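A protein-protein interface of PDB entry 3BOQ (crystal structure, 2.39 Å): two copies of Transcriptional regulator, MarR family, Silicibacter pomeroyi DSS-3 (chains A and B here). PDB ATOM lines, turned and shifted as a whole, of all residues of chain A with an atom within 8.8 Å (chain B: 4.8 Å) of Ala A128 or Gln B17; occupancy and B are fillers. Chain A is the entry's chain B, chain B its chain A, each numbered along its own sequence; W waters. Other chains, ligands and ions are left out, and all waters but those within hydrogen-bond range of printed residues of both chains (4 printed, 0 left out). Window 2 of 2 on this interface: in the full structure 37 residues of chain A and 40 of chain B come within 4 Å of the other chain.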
ATOM      1  N   LEU A  27      24.054  12.779  20.219  1.00  0.00           N
ATOM      2  CA  LEU A  27      24.216  14.216  20.396  1.00  0.00           C
ATOM      3  C   LEU A  27      24.027  14.506  21.893  1.00  0.00           C
ATOM      4  O   LEU A  27      24.848  15.180  22.515  1.00  0.00           O
ATOM      5  CB  LEU A  27      23.249  15.016  19.519  1.00  0.00           C
ATOM      6  CG  LEU A  27      23.428  16.536  19.487  1.00  0.00           C
ATOM      7  CD1 LEU A  27      24.812  16.897  19.033  1.00  0.00           C
ATOM      8  CD2 LEU A  27      22.410  17.199  18.568  1.00  0.00           C
ATOM      9  N   VAL A  31      27.100  16.288  24.080  1.00  0.00           N
ATOM     10  CA  VAL A  31      26.919  17.627  24.607  1.00  0.00           C
ATOM     11  C   VAL A  31      26.934  17.561  26.134  1.00  0.00           C
ATOM     12  O   VAL A  31      27.640  18.328  26.773  1.00  0.00           O
ATOM     13  CB  VAL A  31      25.674  18.320  24.021  1.00  0.00           C
ATOM     14  CG1 VAL A  31      25.323  19.595  24.779  1.00  0.00           C
ATOM     15  CG2 VAL A  31      25.882  18.607  22.524  1.00  0.00           C
ATOM     16  N   LEU A  35      29.575  19.712  28.512  1.00  0.00           N
ATOM     17  CA  LEU A  35      28.874  20.798  29.145  1.00  0.00           C
ATOM     18  C   LEU A  35      28.967  20.634  30.644  1.00  0.00           C
ATOM     19  O   LEU A  35      29.422  21.531  31.317  1.00  0.00           O
ATOM     20  CB  LEU A  35      27.419  20.794  28.709  1.00  0.00           C
ATOM     21  CG  LEU A  35      26.529  21.992  29.004  1.00  0.00           C
ATOM     22  CD1 LEU A  35      27.232  23.325  28.649  1.00  0.00           C
ATOM     23  CD2 LEU A  35      25.200  21.888  28.265  1.00  0.00           C
ATOM     24  N   GLU A 121      25.930  32.530  32.013  1.00  0.00           N
ATOM     25  CA  GLU A 121      26.858  33.085  31.039  1.00  0.00           C
ATOM     26  C   GLU A 121      27.814  31.981  30.570  1.00  0.00           C
ATOM     27  O   GLU A 121      28.002  31.776  29.355  1.00  0.00           O
ATOM     28  CB  GLU A 121      27.634  34.248  31.679  1.00  0.00           C
ATOM     29  CG  GLU A 121      28.082  35.360  30.756  1.00  0.00           C
ATOM     30  CD  GLU A 121      28.398  36.697  31.514  1.00  0.00           C
ATOM     31  OE1 GLU A 121      28.561  36.702  32.781  1.00  0.00           O
ATOM     32  OE2 GLU A 121      28.496  37.753  30.829  1.00  0.00           O
ATOM     33  N   ALA A 122      28.396  31.276  31.544  1.00  0.00           N
ATOM     34  CA  ALA A 122      29.349  30.175  31.324  1.00  0.00           C
ATOM     35  C   ALA A 122      28.758  29.029  30.506  1.00  0.00           C
ATOM     36  O   ALA A 122      29.412  28.496  29.616  1.00  0.00           O
ATOM     37  CB  ALA A 122      29.874  29.645  32.665  1.00  0.00           C
ATOM     38  N   HIS A 123      27.525  28.666  30.839  1.00  0.00           N
ATOM     39  CA  HIS A 123      26.781  27.575  30.206  1.00  0.00           C
ATOM     40  C   HIS A 123      26.572  27.825  28.689  1.00  0.00           C
ATOM     41  O   HIS A 123      26.790  26.918  27.876  1.00  0.00           O
ATOM     42  CB  HIS A 123      25.419  27.441  30.903  1.00  0.00           C
ATOM     43  CG  HIS A 123      24.468  26.523  30.209  1.00  0.00           C
ATOM     44  ND1 HIS A 123      23.729  26.912  29.115  1.00  0.00           N
ATOM     45  CD2 HIS A 123      24.114  25.242  30.468  1.00  0.00           C
ATOM     46  CE1 HIS A 123      22.969  25.905  28.723  1.00  0.00           C
ATOM     47  NE2 HIS A 123      23.188  24.882  29.527  1.00  0.00           N
ATOM     48  N   ASN A 124      26.120  29.039  28.347  1.00  0.00           N
ATOM     49  CA  ASN A 124      25.874  29.441  26.977  1.00  0.00           C
ATOM     50  C   ASN A 124      27.155  29.654  26.180  1.00  0.00           C
ATOM     51  O   ASN A 124      27.173  29.424  24.971  1.00  0.00           O
ATOM     52  CB  ASN A 124      25.014  30.714  26.932  1.00  0.00           C
ATOM     53  CG  ASN A 124      23.603  30.496  27.506  1.00  0.00           C
ATOM     54  OD1 ASN A 124      23.177  29.366  27.729  1.00  0.00           O
ATOM     55  ND2 ASN A 124      22.890  31.578  27.745  1.00  0.00           N
ATOM     56  N   ARG A 125      28.221  30.121  26.829  1.00  0.00           N
ATOM     57  CA  ARG A 125      29.530  30.115  26.200  1.00  0.00           C
ATOM     58  C   ARG A 125      30.027  28.659  25.926  1.00  0.00           C
ATOM     59  O   ARG A 125      30.499  28.362  24.835  1.00  0.00           O
ATOM     60  CB  ARG A 125      30.556  30.944  27.021  1.00  0.00           C
ATOM     61  CG  ARG A 125      31.965  30.909  26.407  1.00  0.00           C
ATOM     62  CD  ARG A 125      33.029  31.754  27.113  1.00  0.00           C
ATOM     63  NE  ARG A 125      32.719  32.021  28.510  1.00  0.00           N
ATOM     64  CZ  ARG A 125      32.894  31.160  29.517  1.00  0.00           C
ATOM     65  NH1 ARG A 125      33.381  29.939  29.294  1.00  0.00           N
ATOM     66  NH2 ARG A 125      32.562  31.520  30.751  1.00  0.00           N
ATOM     67  N   ILE A 126      29.913  27.761  26.905  1.00  0.00           N
ATOM     68  CA  ILE A 126      30.432  26.392  26.730  1.00  0.00           C
ATOM     69  C   ILE A 126      29.689  25.678  25.596  1.00  0.00           C
ATOM     70  O   ILE A 126      30.311  25.043  24.724  1.00  0.00           O
ATOM     71  CB  ILE A 126      30.407  25.562  28.061  1.00  0.00           C
ATOM     72  CG1 ILE A 126      31.399  26.143  29.092  1.00  0.00           C
ATOM     73  CG2 ILE A 126      30.786  24.118  27.820  1.00  0.00           C
ATOM     74  CD1 ILE A 126      30.935  25.964  30.535  1.00  0.00           C
ATOM     75  N   LEU A 127      28.365  25.807  25.604  1.00  0.00           N
ATOM     76  CA  LEU A 127      27.522  25.208  24.587  1.00  0.00           C
ATOM     77  C   LEU A 127      27.869  25.725  23.172  1.00  0.00           C
ATOM     78  O   LEU A 127      28.077  24.908  22.228  1.00  0.00           O
ATOM     79  CB  LEU A 127      26.030  25.397  24.942  1.00  0.00           C
ATOM     80  CG  LEU A 127      24.954  24.714  24.089  1.00  0.00           C
ATOM     81  CD1 LEU A 127      25.017  23.175  24.147  1.00  0.00           C
ATOM     82  CD2 LEU A 127      23.583  25.215  24.546  1.00  0.00           C
ATOM     83  N   ALA A 128      27.957  27.055  23.045  1.00  0.00           N
ATOM     84  CA  ALA A 128      28.424  27.735  21.802  1.00  0.00           C
ATOM     85  C   ALA A 128      29.776  27.196  21.335  1.00  0.00           C
ATOM     86  O   ALA A 128      29.937  26.816  20.167  1.00  0.00           O
ATOM     87  CB  ALA A 128      28.490  29.245  21.980  1.00  0.00           C
ATOM     88  N   GLU A 129      30.720  27.089  22.262  1.00  0.00           N
ATOM     89  CA  GLU A 129      32.013  26.476  21.981  1.00  0.00           C
ATOM     90  C   GLU A 129      31.907  25.012  21.547  1.00  0.00           C
ATOM     91  O   GLU A 129      32.559  24.605  20.586  1.00  0.00           O
ATOM     92  CB  GLU A 129      33.003  26.759  23.130  1.00  0.00           C
ATOM     93  CG  GLU A 129      33.252  28.355  23.297  1.00  0.00           C
ATOM     94  CD  GLU A 129      34.195  28.781  24.447  1.00  0.00           C
ATOM     95  OE1 GLU A 129      34.178  28.186  25.582  1.00  0.00           O
ATOM     96  OE2 GLU A 129      34.948  29.761  24.235  1.00  0.00           O
ATOM     97  N   LEU A 130      31.032  24.222  22.177  1.00  0.00           N
ATOM     98  CA  LEU A 130      30.880  22.809  21.780  1.00  0.00           C
ATOM     99  C   LEU A 130      30.302  22.660  20.370  1.00  0.00           C
ATOM    100  O   LEU A 130      30.601  21.703  19.674  1.00  0.00           O
ATOM    101  CB  LEU A 130      30.003  22.064  22.777  1.00  0.00           C
ATOM    102  CG  LEU A 130      30.612  21.778  24.161  1.00  0.00           C
ATOM    103  CD1 LEU A 130      29.557  21.271  25.176  1.00  0.00           C
ATOM    104  CD2 LEU A 130      31.819  20.824  24.080  1.00  0.00           C
ATOM    105  N   LEU A 131      29.473  23.631  19.976  1.00  0.00           N
ATOM    106  CA  LEU A 131      28.723  23.603  18.735  1.00  0.00           C
ATOM    107  C   LEU A 131      29.301  24.514  17.676  1.00  0.00           C
ATOM    108  O   LEU A 131      28.601  24.895  16.749  1.00  0.00           O
ATOM    109  CB  LEU A 131      27.277  24.023  18.999  1.00  0.00           C
ATOM    110  CG  LEU A 131      26.388  23.123  19.851  1.00  0.00           C
ATOM    111  CD1 LEU A 131      25.025  23.792  19.986  1.00  0.00           C
ATOM    112  CD2 LEU A 131      26.260  21.678  19.244  1.00  0.00           C
ATOM    113  N   ARG A 132      30.592  24.819  17.781  1.00  0.00           N
ATOM    114  CA  ARG A 132      31.177  25.973  17.108  1.00  0.00           C
ATOM    115  C   ARG A 132      31.310  25.786  15.612  1.00  0.00           C
ATOM    116  O   ARG A 132      31.464  26.789  14.864  1.00  0.00           O
ATOM    117  CB  ARG A 132      32.523  26.332  17.722  1.00  0.00           C
ATOM    118  CG  ARG A 132      33.591  25.292  17.467  1.00  0.00           C
ATOM    119  CD  ARG A 132      34.827  25.589  18.228  1.00  0.00           C
ATOM    120  NE  ARG A 132      35.831  24.551  18.051  1.00  0.00           N
ATOM    121  CZ  ARG A 132      35.964  23.477  18.838  1.00  0.00           C
ATOM    122  NH1 ARG A 132      35.128  23.266  19.849  1.00  0.00           N
ATOM    123  NH2 ARG A 132      36.951  22.607  18.605  1.00  0.00           N
ATOM    124  N   ALA A 133      31.244  24.519  15.184  1.00  0.00           N
ATOM    125  CA  ALA A 133      31.410  24.164  13.776  1.00  0.00           C
ATOM    126  C   ALA A 133      30.054  23.838  13.211  1.00  0.00           C
ATOM    127  O   ALA A 133      29.889  23.588  12.016  1.00  0.00           O
ATOM    128  CB  ALA A 133      32.368  22.985  13.618  1.00  0.00           C
ATOM    129  N   VAL A 134      29.059  23.828  14.068  1.00  0.00           N
ATOM    130  CA  VAL A 134      27.715  23.470  13.622  1.00  0.00           C
ATOM    131  C   VAL A 134      27.071  24.661  12.893  1.00  0.00           C
ATOM    132  O   VAL A 134      27.160  25.832  13.317  1.00  0.00           O
ATOM    133  CB  VAL A 134      26.876  22.904  14.781  1.00  0.00           C
ATOM    134  CG1 VAL A 134      25.536  22.383  14.294  1.00  0.00           C
ATOM    135  CG2 VAL A 134      27.652  21.767  15.480  1.00  0.00           C
ATOM    136  N   SER A 135      26.478  24.357  11.752  1.00  0.00           N
ATOM    137  CA  SER A 135      25.816  25.355  10.968  1.00  0.00           C
ATOM    138  C   SER A 135      24.429  25.730  11.522  1.00  0.00           C
ATOM    139  O   SER A 135      23.692  24.879  12.031  1.00  0.00           O
ATOM    140  CB  SER A 135      25.700  24.870   9.526  1.00  0.00           C
ATOM    141  OG  SER A 135      24.650  23.960   9.473  1.00  0.00           O
ATOM    142  N   ASP A 136      24.071  26.998  11.385  1.00  0.00           N
ATOM    143  CA  ASP A 136      22.740  27.463  11.729  1.00  0.00           C
ATOM    144  C   ASP A 136      21.654  26.643  11.065  1.00  0.00           C
ATOM    145  O   ASP A 136      20.701  26.284  11.731  1.00  0.00           O
ATOM    146  CB  ASP A 136      22.548  28.918  11.332  1.00  0.00           C
ATOM    147  CG  ASP A 136      23.329  29.875  12.196  1.00  0.00           C
ATOM    148  OD1 ASP A 136      23.661  29.548  13.343  1.00  0.00           O
ATOM    149  OD2 ASP A 136      23.555  31.015  11.742  1.00  0.00           O
ATOM    150  N   MET A 139      20.989  23.253  12.705  1.00  0.00           N
ATOM    151  CA  MET A 139      20.379  23.463  14.019  1.00  0.00           C
ATOM    152  C   MET A 139      18.905  23.830  13.900  1.00  0.00           C
ATOM    153  O   MET A 139      18.081  23.261  14.602  1.00  0.00           O
ATOM    154  CB  MET A 139      21.092  24.576  14.792  1.00  0.00           C
ATOM    155  CG  MET A 139      22.416  24.172  15.359  1.00  0.00           C
ATOM    156  SD  MET A 139      23.071  25.476  16.656  1.00  0.00           S
ATOM    157  CE  MET A 139      23.678  26.847  15.440  1.00  0.00           C
ATOM    158  N   VAL A 140      18.592  24.798  13.024  1.00  0.00           N
ATOM    159  CA  VAL A 140      17.220  25.191  12.691  1.00  0.00           C
ATOM    160  C   VAL A 140      16.408  23.985  12.170  1.00  0.00           C
ATOM    161  O   VAL A 140      15.274  23.780  12.600  1.00  0.00           O
ATOM    162  CB  VAL A 140      17.190  26.403  11.703  1.00  0.00           C
ATOM    163  CG1 VAL A 140      15.778  26.741  11.287  1.00  0.00           C
ATOM    164  CG2 VAL A 140      17.828  27.631  12.352  1.00  0.00           C
ATOM    165  N   SER A 143      15.962  21.330  14.981  1.00  0.00           N
ATOM    166  CA  SER A 143      14.983  21.826  15.880  1.00  0.00           C
ATOM    167  C   SER A 143      13.545  21.793  15.327  1.00  0.00           C
ATOM    168  O   SER A 143      12.633  21.393  16.045  1.00  0.00           O
ATOM    169  CB  SER A 143      15.345  23.231  16.300  1.00  0.00           C
ATOM    170  OG  SER A 143      15.240  23.302  17.680  1.00  0.00           O
ATOM    171  N   ARG B  13      21.666  33.071  16.687  1.00  0.00           N
ATOM    172  CA  ARG B  13      22.400  31.803  16.779  1.00  0.00           C
ATOM    173  C   ARG B  13      22.325  31.219  18.198  1.00  0.00           C
ATOM    174  O   ARG B  13      22.145  30.015  18.362  1.00  0.00           O
ATOM    175  CB  ARG B  13      23.874  31.986  16.371  1.00  0.00           C
ATOM    176  CG  ARG B  13      24.741  30.735  16.579  1.00  0.00           C
ATOM    177  CD  ARG B  13      25.910  30.624  15.629  1.00  0.00           C
ATOM    178  NE  ARG B  13      26.694  29.458  15.992  1.00  0.00           N
ATOM    179  CZ  ARG B  13      26.675  28.272  15.375  1.00  0.00           C
ATOM    180  NH1 ARG B  13      25.940  28.069  14.275  1.00  0.00           N
ATOM    181  NH2 ARG B  13      27.432  27.285  15.849  1.00  0.00           N
ATOM    182  N   GLN B  14      22.466  32.074  19.218  1.00  0.00           N
ATOM    183  CA  GLN B  14      22.380  31.629  20.615  1.00  0.00           C
ATOM    184  C   GLN B  14      20.997  31.089  20.953  1.00  0.00           C
ATOM    185  O   GLN B  14      20.899  30.055  21.580  1.00  0.00           O
ATOM    186  CB  GLN B  14      22.827  32.716  21.605  1.00  0.00           C
ATOM    187  CG  GLN B  14      23.881  33.539  21.009  1.00  0.00           C
ATOM    188  CD  GLN B  14      24.619  34.452  21.992  1.00  0.00           C
ATOM    189  OE1 GLN B  14      24.191  35.580  22.279  1.00  0.00           O
ATOM    190  NE2 GLN B  14      25.762  33.960  22.489  1.00  0.00           N
ATOM    191  N   GLN B  15      19.942  31.763  20.514  1.00  0.00           N
ATOM    192  CA  GLN B  15      18.587  31.241  20.643  1.00  0.00           C
ATOM    193  C   GLN B  15      18.418  29.894  19.938  1.00  0.00           C
ATOM    194  O   GLN B  15      17.876  28.973  20.509  1.00  0.00           O
ATOM    195  CB  GLN B  15      17.558  32.267  20.157  1.00  0.00           C
ATOM    196  CG  GLN B  15      17.504  33.504  21.029  1.00  0.00           C
ATOM    197  CD  GLN B  15      16.495  34.562  20.548  1.00  0.00           C
ATOM    198  OE1 GLN B  15      16.870  35.588  19.965  1.00  0.00           O
ATOM    199  NE2 GLN B  15      15.215  34.319  20.810  1.00  0.00           N
ATOM    200  N   ASN B  16      18.915  29.752  18.718  1.00  0.00           N
ATOM    201  CA  ASN B  16      18.824  28.461  18.029  1.00  0.00           C
ATOM    202  C   ASN B  16      19.540  27.326  18.771  1.00  0.00           C
ATOM    203  O   ASN B  16      19.113  26.179  18.666  1.00  0.00           O
ATOM    204  CB  ASN B  16      19.371  28.527  16.591  1.00  0.00           C
ATOM    205  CG  ASN B  16      18.655  29.551  15.735  1.00  0.00           C
ATOM    206  OD1 ASN B  16      17.477  29.845  15.942  1.00  0.00           O
ATOM    207  ND2 ASN B  16      19.367  30.097  14.753  1.00  0.00           N
ATOM    208  N   GLN B  17      20.632  27.632  19.484  1.00  0.00           N
ATOM    209  CA  GLN B  17      21.413  26.598  20.198  1.00  0.00           C
ATOM    210  C   GLN B  17      20.654  26.178  21.441  1.00  0.00           C
ATOM    211  O   GLN B  17      20.562  24.989  21.740  1.00  0.00           O
ATOM    212  CB  GLN B  17      22.804  27.111  20.592  1.00  0.00           C
ATOM    213  CG  GLN B  17      23.710  27.382  19.380  1.00  0.00           C
ATOM    214  CD  GLN B  17      25.044  28.006  19.715  1.00  0.00           C
ATOM    215  OE1 GLN B  17      25.234  28.560  20.795  1.00  0.00           O
ATOM    216  NE2 GLN B  17      25.989  27.911  18.784  1.00  0.00           N
ATOM    217  N   THR B  18      20.141  27.162  22.178  1.00  0.00           N
ATOM    218  CA  THR B  18      19.267  26.902  23.324  1.00  0.00           C
ATOM    219  C   THR B  18      18.029  26.101  22.919  1.00  0.00           C
ATOM    220  O   THR B  18      17.643  25.188  23.605  1.00  0.00           O
ATOM    221  CB  THR B  18      18.792  28.237  23.981  1.00  0.00           C
ATOM    222  OG1 THR B  18      19.895  28.842  24.626  1.00  0.00           O
ATOM    223  CG2 THR B  18      17.677  28.022  25.033  1.00  0.00           C
ATOM    224  N   ARG B  19      17.391  26.495  21.828  1.00  0.00           N
ATOM    225  CA  ARG B  19      16.198  25.837  21.353  1.00  0.00           C
ATOM    226  C   ARG B  19      16.516  24.371  20.991  1.00  0.00           C
ATOM    227  O   ARG B  19      15.749  23.466  21.291  1.00  0.00           O
ATOM    228  CB  ARG B  19      15.691  26.621  20.147  1.00  0.00           C
ATOM    229  CG  ARG B  19      14.232  26.531  19.807  1.00  0.00           C
ATOM    230  CD  ARG B  19      13.927  27.522  18.652  1.00  0.00           C
ATOM    231  NE  ARG B  19      13.532  28.842  19.156  1.00  0.00           N
ATOM    232  CZ  ARG B  19      14.119  30.010  18.867  1.00  0.00           C
ATOM    233  NH1 ARG B  19      15.169  30.085  18.037  1.00  0.00           N
ATOM    234  NH2 ARG B  19      13.636  31.126  19.410  1.00  0.00           N
ATOM    235  N   LEU B  20      17.663  24.144  20.369  1.00  0.00           N
ATOM    236  CA  LEU B  20      18.056  22.819  19.922  1.00  0.00           C
ATOM    237  C   LEU B  20      18.322  21.936  21.120  1.00  0.00           C
ATOM    238  O   LEU B  20      17.788  20.842  21.238  1.00  0.00           O
ATOM    239  CB  LEU B  20      19.319  22.912  19.065  1.00  0.00           C
ATOM    240  CG  LEU B  20      19.961  21.550  18.765  1.00  0.00           C
ATOM    241  CD1 LEU B  20      19.012  20.707  17.910  1.00  0.00           C
ATOM    242  CD2 LEU B  20      21.362  21.698  18.127  1.00  0.00           C
ATOM    243  N   TRP B  21      19.106  22.444  22.046  1.00  0.00           N
ATOM    244  CA  TRP B  21      19.465  21.701  23.224  1.00  0.00           C
ATOM    245  C   TRP B  21      18.258  21.377  24.131  1.00  0.00           C
ATOM    246  O   TRP B  21      18.123  20.246  24.577  1.00  0.00           O
ATOM    247  CB  TRP B  21      20.546  22.463  23.945  1.00  0.00           C
ATOM    248  CG  TRP B  21      21.033  21.859  25.212  1.00  0.00           C
ATOM    249  CD1 TRP B  21      21.155  22.504  26.391  1.00  0.00           C
ATOM    250  CD2 TRP B  21      21.498  20.507  25.432  1.00  0.00           C
ATOM    251  NE1 TRP B  21      21.659  21.656  27.333  1.00  0.00           N
ATOM    252  CE2 TRP B  21      21.876  20.424  26.780  1.00  0.00           C
ATOM    253  CE3 TRP B  21      21.635  19.371  24.618  1.00  0.00           C
ATOM    254  CZ2 TRP B  21      22.383  19.251  27.356  1.00  0.00           C
ATOM    255  CZ3 TRP B  21      22.125  18.194  25.190  1.00  0.00           C
ATOM    256  CH2 TRP B  21      22.490  18.145  26.550  1.00  0.00           C
HETATM  257  O   HOH W   1      28.487  28.537  18.351  1.00  0.00           O
HETATM  258  O   HOH W   2      24.677  28.562  23.266  1.00  0.00           O
HETATM  259  O   HOH W   3      21.488  28.905  14.647  1.00  0.00           O
HETATM  260  O   HOH W   4      17.480  25.631  16.761  1.00  0.00           O
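O of Leu A131 sits at hydrogen-bond distance from NH2 of Arg B13 (2.8 Å).
The guanidinium group (NH1) of Arg B13 is in hydrogen-bond range of the backbone carbonyl oxygen (O) of Val A134.
NH1 of Arg B13 lies within salt-bridge range of OD1 of Asp A136 (2.9 Å).
NE2 of Gln B17 lies close to NE of Arg B13.
The side-chain amide oxygen of Asn B16 is in hydrogen-bond range of the guanidinium group of Arg B19 (3.1 Å).
Among the printed residues, merely in contact across the chains: Val A31 with Trp B21 (3.5 Å), Leu A35 with Trp B21 (3.7 Å), Ala A128 with Gln B17 (3.4 Å), Leu A131 with Gln B17 (3.9 Å), Ser A135 with Arg B13 (3.9 Å), Met A139 with Arg B13 (2.8 Å), Met A139 with Gln B17 (3.4 Å), Met A139 with Leu B20 (3.9 Å), Val A140 with Asn B16 (3.8 Å), Ser A143 with Arg B19 (3.7 Å) and Ser A143 with Leu B20 (3.6 Å).
Of the printed residues of chain B, Ala A128 touches Gln B17 (3.4 Å).
Gln B17 touches three residues of chain A.
Of the printed residues of chain B, Val A140 touches Asn B16 (3.8 Å).
Of the printed residues of chain A, Arg B13 touches Leu A131 (2.8 Å), Val A134 (2.7 Å), Ser A135 (3.9 Å), Asp A136 (2.9 Å) and Met A139 (2.8 Å).
Of the printed residues of chain A, Leu B20 touches Met A139 (3.9 Å) and Ser A143 (3.6 Å).
Of the printed residues of chain B, Leu A131 touches Arg B13 and Gln B17.
Printed residues of chain A within 4 Å of Asn B16: Val A140.
Arg A125 touches none of the printed residues of chain B.
The nearest residue of chain A that does not touch Gln B17 is Leu A127 (4.1 Å).
Of the 22 printed residues of chain A, 10 touch a printed residue of chain B.
Hydrophobic or aromatic side chains of chain B within 4 Å of the printed part of chain A: Leu B20 and Trp B21.
Along chain B the printed residues that touch a printed residue of chain A span positions 13 to 21.
Among the printed residues, Asp or Glu carboxylates within 4 Å of a Lys or Arg side-chain nitrogen of the other chain: Asp A136 with Arg B13.
No position is printed for both chains.
Of the 14 pairs that touch across the chains among the printed residues, none has its exchanged pair printed and touching as well.
Water W3 bridges the side-chain amide nitrogen (ND2) of Asn B16 and the side-chain carboxylate (OD1) of Asp A136.
Water W2 lies within hydrogen-bond range of the side-chain amide oxygen of Gln B17 (2.5 Å) and the backbone carbonyl oxygen of Asn A124 (3.1 Å).
Water W4 lies within hydrogen-bond range of the backbone carbonyl oxygen of Asn B16 (2.6 Å), the backbone carbonyl oxygen of Met A139 (3.3 Å) and the side-chain hydroxyl of Ser A143 (3.4 Å).
Water W1 lies within hydrogen-bond range of the side-chain amide nitrogen (NE2) of Gln B17, the backbone carbonyl oxygen (O) of Ala A128 and the guanidinium group (NH2) of Arg B13.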
